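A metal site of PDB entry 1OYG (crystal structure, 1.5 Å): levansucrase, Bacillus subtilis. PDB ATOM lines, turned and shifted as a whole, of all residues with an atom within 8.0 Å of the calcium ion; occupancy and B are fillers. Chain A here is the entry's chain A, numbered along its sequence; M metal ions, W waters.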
ATOM      1  N   GLN A 200       1.957   6.229   8.389  1.00  0.00           N
ATOM      2  CA  GLN A 200       0.676   6.743   8.822  1.00  0.00           C
ATOM      3  C   GLN A 200       0.750   7.276  10.254  1.00  0.00           C
ATOM      4  O   GLN A 200       1.449   6.714  11.089  1.00  0.00           O
ATOM      5  CB  GLN A 200      -0.388   5.638   8.732  1.00  0.00           C
ATOM      6  CG  GLN A 200      -1.831   6.115   8.802  1.00  0.00           C
ATOM      7  CD  GLN A 200      -2.830   4.973   8.900  1.00  0.00           C
ATOM      8  OE1 GLN A 200      -2.670   4.067   9.718  1.00  0.00           O
ATOM      9  NE2 GLN A 200      -3.873   5.017   8.060  1.00  0.00           N
ATOM     10  N   PHE A 205      -5.731   8.072  10.696  1.00  0.00           N
ATOM     11  CA  PHE A 205      -6.679   7.078  11.213  1.00  0.00           C
ATOM     12  C   PHE A 205      -8.002   7.723  11.592  1.00  0.00           C
ATOM     13  O   PHE A 205      -9.080   7.210  11.268  1.00  0.00           O
ATOM     14  CB  PHE A 205      -6.047   6.387  12.428  1.00  0.00           C
ATOM     15  CG  PHE A 205      -6.884   5.305  13.049  1.00  0.00           C
ATOM     16  CD1 PHE A 205      -7.316   4.219  12.308  1.00  0.00           C
ATOM     17  CD2 PHE A 205      -7.185   5.347  14.397  1.00  0.00           C
ATOM     18  CE1 PHE A 205      -8.055   3.209  12.903  1.00  0.00           C
ATOM     19  CE2 PHE A 205      -7.922   4.340  15.001  1.00  0.00           C
ATOM     20  CZ  PHE A 205      -8.360   3.275  14.253  1.00  0.00           C
ATOM     21  N   GLU A 208     -10.325   8.738   8.692  1.00  0.00           N
ATOM     22  CA  GLU A 208     -11.095   7.626   8.111  1.00  0.00           C
ATOM     23  C   GLU A 208     -12.338   7.250   8.929  1.00  0.00           C
ATOM     24  O   GLU A 208     -13.214   6.542   8.424  1.00  0.00           O
ATOM     25  CB  GLU A 208     -10.214   6.380   7.963  1.00  0.00           C
ATOM     26  CG  GLU A 208      -8.940   6.581   7.151  1.00  0.00           C
ATOM     27  CD  GLU A 208      -9.101   6.381   5.650  1.00  0.00           C
ATOM     28  OE1 GLU A 208     -10.236   6.097   5.191  1.00  0.00           O
ATOM     29  OE2 GLU A 208      -8.085   6.509   4.926  1.00  0.00           O
ATOM     30  N   SER A 213     -14.132   2.447  10.938  1.00  0.00           N
ATOM     31  CA  SER A 213     -13.756   2.423   9.526  1.00  0.00           C
ATOM     32  C   SER A 213     -13.239   1.061   9.075  1.00  0.00           C
ATOM     33  O   SER A 213     -13.206   0.770   7.892  1.00  0.00           O
ATOM     34  CB  SER A 213     -12.672   3.482   9.257  1.00  0.00           C
ATOM     35  OG  SER A 213     -11.419   3.094   9.783  1.00  0.00           O
ATOM     36  N   GLY A 214     -12.808   0.230  10.027  1.00  0.00           N
ATOM     37  CA  GLY A 214     -12.138  -1.027   9.722  1.00  0.00           C
ATOM     38  C   GLY A 214     -10.638  -0.888   9.511  1.00  0.00           C
ATOM     39  O   GLY A 214      -9.937  -1.884   9.402  1.00  0.00           O
ATOM     40  N   ASP A 215     -10.141   0.346   9.448  1.00  0.00           N
ATOM     41  CA  ASP A 215      -8.711   0.588   9.350  1.00  0.00           C
ATOM     42  C   ASP A 215      -8.041   0.161  10.645  1.00  0.00           C
ATOM     43  O   ASP A 215      -8.676   0.115  11.703  1.00  0.00           O
ATOM     44  CB  ASP A 215      -8.426   2.074   9.077  1.00  0.00           C
ATOM     45  CG  ASP A 215      -7.054   2.323   8.452  1.00  0.00           C
ATOM     46  OD1 ASP A 215      -6.440   1.365   7.925  1.00  0.00           O
ATOM     47  OD2 ASP A 215      -6.520   3.449   8.446  1.00  0.00           O
ATOM     48  N   ASN A 216      -6.761  -0.182  10.558  1.00  0.00           N
ATOM     49  CA  ASN A 216      -5.990  -0.649  11.692  1.00  0.00           C
ATOM     50  C   ASN A 216      -4.675   0.119  11.723  1.00  0.00           C
ATOM     51  O   ASN A 216      -3.730  -0.200  10.995  1.00  0.00           O
ATOM     52  CB  ASN A 216      -5.761  -2.156  11.593  1.00  0.00           C
ATOM     53  CG  ASN A 216      -4.970  -2.710  12.758  1.00  0.00           C
ATOM     54  OD1 ASN A 216      -4.703  -1.999  13.730  1.00  0.00           O
ATOM     55  ND2 ASN A 216      -4.571  -3.979  12.665  1.00  0.00           N
ATOM     56  N   HIS A 217      -4.627   1.143  12.573  1.00  0.00           N
ATOM     57  CA  HIS A 217      -3.465   2.000  12.681  1.00  0.00           C
ATOM     58  C   HIS A 217      -2.462   1.424  13.678  1.00  0.00           C
ATOM     59  O   HIS A 217      -2.827   1.063  14.798  1.00  0.00           O
ATOM     60  CB  HIS A 217      -3.856   3.395  13.124  1.00  0.00           C
ATOM     61  CG  HIS A 217      -2.683   4.274  13.411  1.00  0.00           C
ATOM     62  ND1 HIS A 217      -1.833   4.729  12.419  1.00  0.00           N
ATOM     63  CD2 HIS A 217      -2.175   4.742  14.580  1.00  0.00           C
ATOM     64  CE1 HIS A 217      -0.877   5.463  12.968  1.00  0.00           C
ATOM     65  NE2 HIS A 217      -1.054   5.475  14.268  1.00  0.00           N
ATOM     66  N   THR A 218      -1.204   1.367  13.251  1.00  0.00           N
ATOM     67  CA  THR A 218      -0.126   0.834  14.060  1.00  0.00           C
ATOM     68  C   THR A 218       1.123   1.707  13.921  1.00  0.00           C
ATOM     69  O   THR A 218       1.398   2.253  12.851  1.00  0.00           O
ATOM     70  CB  THR A 218       0.223  -0.621  13.655  1.00  0.00           C
ATOM     71  OG1 THR A 218       0.970  -0.634  12.430  1.00  0.00           O
ATOM     72  CG2 THR A 218      -1.032  -1.444  13.336  1.00  0.00           C
ATOM     73  N   ALA A 237       4.552  -0.464  11.346  1.00  0.00           N
ATOM     74  CA  ALA A 237       3.869   0.761  10.947  1.00  0.00           C
ATOM     75  C   ALA A 237       2.885   0.479   9.833  1.00  0.00           C
ATOM     76  O   ALA A 237       2.558  -0.678   9.541  1.00  0.00           O
ATOM     77  CB  ALA A 237       4.899   1.799  10.500  1.00  0.00           C
ATOM     78  N   ASN A 238       2.366   1.556   9.255  1.00  0.00           N
ATOM     79  CA  ASN A 238       1.573   1.487   8.037  1.00  0.00           C
ATOM     80  C   ASN A 238       2.121   2.546   7.097  1.00  0.00           C
ATOM     81  O   ASN A 238       2.683   3.533   7.558  1.00  0.00           O
ATOM     82  CB  ASN A 238       0.093   1.720   8.345  1.00  0.00           C
ATOM     83  CG  ASN A 238      -0.445   0.684   9.284  1.00  0.00           C
ATOM     84  OD1 ASN A 238      -0.375   0.842  10.503  1.00  0.00           O
ATOM     85  ND2 ASN A 238      -0.960  -0.408   8.740  1.00  0.00           N
ATOM     86  N   THR A 239       1.980   2.339   5.796  1.00  0.00           N
ATOM     87  CA  THR A 239       2.496   3.326   4.850  1.00  0.00           C
ATOM     88  C   THR A 239       1.764   4.648   4.966  1.00  0.00           C
ATOM     89  O   THR A 239       0.655   4.722   5.510  1.00  0.00           O
ATOM     90  CB  THR A 239       2.406   2.830   3.396  1.00  0.00           C
ATOM     91  OG1 THR A 239       1.041   2.546   3.075  1.00  0.00           O
ATOM     92  CG2 THR A 239       3.163   1.519   3.200  1.00  0.00           C
ATOM     93  N   TYR A 245      -0.028   4.346  -0.335  1.00  0.00           N
ATOM     94  CA  TYR A 245      -1.032   4.426   0.715  1.00  0.00           C
ATOM     95  C   TYR A 245      -2.174   3.459   0.478  1.00  0.00           C
ATOM     96  O   TYR A 245      -2.383   2.984  -0.644  1.00  0.00           O
ATOM     97  CB  TYR A 245      -1.572   5.856   0.840  1.00  0.00           C
ATOM     98  CG  TYR A 245      -2.204   6.195   2.185  1.00  0.00           C
ATOM     99  CD1 TYR A 245      -1.578   5.862   3.375  1.00  0.00           C
ATOM    100  CD2 TYR A 245      -3.436   6.851   2.250  1.00  0.00           C
ATOM    101  CE1 TYR A 245      -2.149   6.159   4.607  1.00  0.00           C
ATOM    102  CE2 TYR A 245      -4.013   7.168   3.476  1.00  0.00           C
ATOM    103  CZ  TYR A 245      -3.372   6.819   4.645  1.00  0.00           C
ATOM    104  OH  TYR A 245      -3.945   7.125   5.863  1.00  0.00           O
ATOM    105  N   GLN A 246      -2.887   3.155   1.557  1.00  0.00           N
ATOM    106  CA  GLN A 246      -4.160   2.460   1.482  1.00  0.00           C
ATOM    107  C   GLN A 246      -5.117   3.225   0.572  1.00  0.00           C
ATOM    108  O   GLN A 246      -4.976   4.443   0.387  1.00  0.00           O
ATOM    109  CB  GLN A 246      -4.769   2.296   2.876  1.00  0.00           C
ATOM    110  CG  GLN A 246      -5.110   3.625   3.580  1.00  0.00           C
ATOM    111  CD  GLN A 246      -5.321   3.456   5.068  1.00  0.00           C
ATOM    112  OE1 GLN A 246      -4.646   2.639   5.703  1.00  0.00           O
ATOM    113  NE2 GLN A 246      -6.253   4.211   5.631  1.00  0.00           N
ATOM    114  N   GLY A 247      -6.083   2.508   0.007  1.00  0.00           N
ATOM    115  CA  GLY A 247      -7.093   3.113  -0.831  1.00  0.00           C
ATOM    116  C   GLY A 247      -7.556   2.177  -1.941  1.00  0.00           C
ATOM    117  O   GLY A 247      -7.012   1.094  -2.134  1.00  0.00           O
ATOM    118  N   THR A 279     -11.105  -4.868   2.979  1.00  0.00           N
ATOM    119  CA  THR A 279     -10.005  -5.219   3.875  1.00  0.00           C
ATOM    120  C   THR A 279      -8.660  -5.020   3.167  1.00  0.00           C
ATOM    121  O   THR A 279      -7.709  -4.493   3.737  1.00  0.00           O
ATOM    122  CB  THR A 279     -10.134  -6.680   4.373  1.00  0.00           C
ATOM    123  OG1 THR A 279     -11.369  -6.846   5.089  1.00  0.00           O
ATOM    124  CG2 THR A 279      -9.048  -7.028   5.383  1.00  0.00           C
ATOM    125  N   ALA A 280      -8.617  -5.409   1.898  1.00  0.00           N
ATOM    126  CA  ALA A 280      -7.402  -5.288   1.093  1.00  0.00           C
ATOM    127  C   ALA A 280      -7.059  -3.833   0.804  1.00  0.00           C
ATOM    128  O   ALA A 280      -5.904  -3.441   0.850  1.00  0.00           O
ATOM    129  CB  ALA A 280      -7.539  -6.076  -0.201  1.00  0.00           C
ATOM    130  N   GLU A 281      -8.078  -3.023   0.501  1.00  0.00           N
ATOM    131  CA  GLU A 281      -7.879  -1.596   0.267  1.00  0.00           C
ATOM    132  C   GLU A 281      -7.298  -0.902   1.500  1.00  0.00           C
ATOM    133  O   GLU A 281      -6.435  -0.051   1.385  1.00  0.00           O
ATOM    134  CB  GLU A 281      -9.192  -0.934  -0.142  1.00  0.00           C
ATOM    135  CG  GLU A 281      -9.675  -1.344  -1.535  1.00  0.00           C
ATOM    136  CD  GLU A 281     -11.120  -0.975  -1.826  1.00  0.00           C
ATOM    137  OE1 GLU A 281     -11.882  -0.663  -0.891  1.00  0.00           O
ATOM    138  OE2 GLU A 281     -11.505  -1.006  -3.014  1.00  0.00           O
ATOM    139  N   LEU A 282      -7.761  -1.302   2.689  1.00  0.00           N
ATOM    140  CA  LEU A 282      -7.297  -0.725   3.950  1.00  0.00           C
ATOM    141  C   LEU A 282      -5.929  -1.242   4.360  1.00  0.00           C
ATOM    142  O   LEU A 282      -5.234  -0.605   5.142  1.00  0.00           O
ATOM    143  CB  LEU A 282      -8.285  -1.015   5.072  1.00  0.00           C
ATOM    144  CG  LEU A 282      -9.616  -0.264   5.014  1.00  0.00           C
ATOM    145  CD1 LEU A 282     -10.667  -0.977   5.860  1.00  0.00           C
ATOM    146  CD2 LEU A 282      -9.437   1.177   5.479  1.00  0.00           C
ATOM    147  N   ALA A 283      -5.543  -2.407   3.843  1.00  0.00           N
ATOM    148  CA  ALA A 283      -4.307  -3.070   4.265  1.00  0.00           C
ATOM    149  C   ALA A 283      -3.067  -2.390   3.691  1.00  0.00           C
ATOM    150  O   ALA A 283      -2.842  -2.387   2.483  1.00  0.00           O
ATOM    151  CB  ALA A 283      -4.324  -4.535   3.840  1.00  0.00           C
ATOM    152  N   ASN A 284      -2.251  -1.805   4.571  1.00  0.00           N
ATOM    153  CA  ASN A 284      -1.012  -1.157   4.157  1.00  0.00           C
ATOM    154  C   ASN A 284       0.042  -1.235   5.256  1.00  0.00           C
ATOM    155  O   ASN A 284       0.713  -0.264   5.577  1.00  0.00           O
ATOM    156  CB  ASN A 284      -1.269   0.285   3.706  1.00  0.00           C
ATOM    157  CG  ASN A 284      -1.667   1.229   4.838  1.00  0.00           C
ATOM    158  OD1 ASN A 284      -2.354   0.834   5.777  1.00  0.00           O
ATOM    159  ND2 ASN A 284      -1.238   2.477   4.733  1.00  0.00           N
ATOM    160  N   GLY A 285       0.219  -2.422   5.815  1.00  0.00           N
ATOM    161  CA  GLY A 285       1.252  -2.672   6.801  1.00  0.00           C
ATOM    162  C   GLY A 285       2.641  -2.395   6.261  1.00  0.00           C
ATOM    163  O   GLY A 285       2.883  -2.443   5.058  1.00  0.00           O
ATOM    164  N   ASN A 309       0.935  -4.097   1.468  1.00  0.00           N
ATOM    165  CA  ASN A 309      -0.267  -3.586   0.818  1.00  0.00           C
ATOM    166  C   ASN A 309      -1.131  -4.701   0.244  1.00  0.00           C
ATOM    167  O   ASN A 309      -0.625  -5.614  -0.416  1.00  0.00           O
ATOM    168  CB  ASN A 309       0.074  -2.621  -0.313  1.00  0.00           C
ATOM    169  CG  ASN A 309       0.738  -1.347   0.176  1.00  0.00           C
ATOM    170  OD1 ASN A 309       1.947  -1.304   0.376  1.00  0.00           O
ATOM    171  ND2 ASN A 309      -0.056  -0.268   0.312  1.00  0.00           N
ATOM    172  N   THR A 312      -2.192  -7.470   4.361  1.00  0.00           N
ATOM    173  CA  THR A 312      -2.598  -7.207   5.738  1.00  0.00           C
ATOM    174  C   THR A 312      -2.182  -5.820   6.210  1.00  0.00           C
ATOM    175  O   THR A 312      -1.230  -5.229   5.704  1.00  0.00           O
ATOM    176  CB  THR A 312      -2.026  -8.292   6.675  1.00  0.00           C
ATOM    177  OG1 THR A 312      -2.438  -8.023   8.029  1.00  0.00           O
ATOM    178  CG2 THR A 312      -0.517  -8.242   6.725  1.00  0.00           C
ATOM    179  N   ASP A 313      -2.913  -5.335   7.209  1.00  0.00           N
ATOM    180  CA  ASP A 313      -2.630  -4.060   7.847  1.00  0.00           C
ATOM    181  C   ASP A 313      -1.721  -4.226   9.061  1.00  0.00           C
ATOM    182  O   ASP A 313      -1.281  -3.237   9.648  1.00  0.00           O
ATOM    183  CB  ASP A 313      -3.946  -3.436   8.323  1.00  0.00           C
ATOM    184  CG  ASP A 313      -4.095  -1.980   7.946  1.00  0.00           C
ATOM    185  OD1 ASP A 313      -3.182  -1.400   7.321  1.00  0.00           O
ATOM    186  OD2 ASP A 313      -5.118  -1.333   8.232  1.00  0.00           O
ATOM    187  N   GLU A 314      -1.424  -5.465   9.448  1.00  0.00           N
ATOM    188  CA  GLU A 314      -0.799  -5.758  10.733  1.00  0.00           C
ATOM    189  C   GLU A 314       0.331  -6.773  10.615  1.00  0.00           C
ATOM    190  O   GLU A 314       0.100  -7.981  10.586  1.00  0.00           O
ATOM    191  CB  GLU A 314      -1.854  -6.252  11.714  1.00  0.00           C
ATOM    192  CG  GLU A 314      -1.389  -6.314  13.154  1.00  0.00           C
ATOM    193  CD  GLU A 314      -2.516  -6.690  14.084  1.00  0.00           C
ATOM    194  OE1 GLU A 314      -3.226  -5.774  14.545  1.00  0.00           O
ATOM    195  OE2 GLU A 314      -2.719  -7.900  14.341  1.00  0.00           O
HETATM  196 CA    CA M   1      -4.422   0.689   6.908  1.00  0.00          CA
HETATM  197  O   HOH W   1      -3.420   1.557   8.852  1.00  0.00           O
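NE2 of Gln 246 is in hydrogen-bond range of OE2 of Glu 208 (3.0 Å). OD2 of Asp 215 is in hydrogen-bond range of NE2 of Gln 200 (3.1 Å). OG of Ser 213 is in hydrogen-bond range of N of Asp 215 (3.0 Å). The side-chain amide nitrogen (ND2) of Asn 238 is in hydrogen-bond range of the backbone carbonyl oxygen (O) of Asp 313. The backbone NH (N) of Asn 216 lies close to the side-chain carboxylate (OD2) of Asp 313. The side-chain amide nitrogen (NE2) of Gln 246 sits close to the side-chain amide nitrogen (NE2) of Gln 200 (3.5 Å). ND2 of Asn 284 lies within hydrogen-bond range of OG1 of Thr 239 (2.8 Å).
OE1 of Gln 246 binds the calcium ion (2.3 Å). The calcium ion is bound by the backbone carbonyl oxygen (O) of Leu 282. Water W1 is bound to the calcium ion. The side-chain carboxylate (OD1) of Asp 215 binds the calcium ion (2.4 Å). The calcium ion is bound by OD1 of Asn 284 (2.4 Å). OD1 of Asp 313 binds the calcium ion (2.5 Å). OD2 of Asp 313 is bound to the calcium ion (2.5 Å). The calcium ion has seven donor atoms within binding distance.
Water W1 lies within hydrogen-bond range of OE1 of Gln 200 (2.8 Å), O of Asn 216 (2.8 Å) and ND2 of Asn 238 (3.2 Å).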
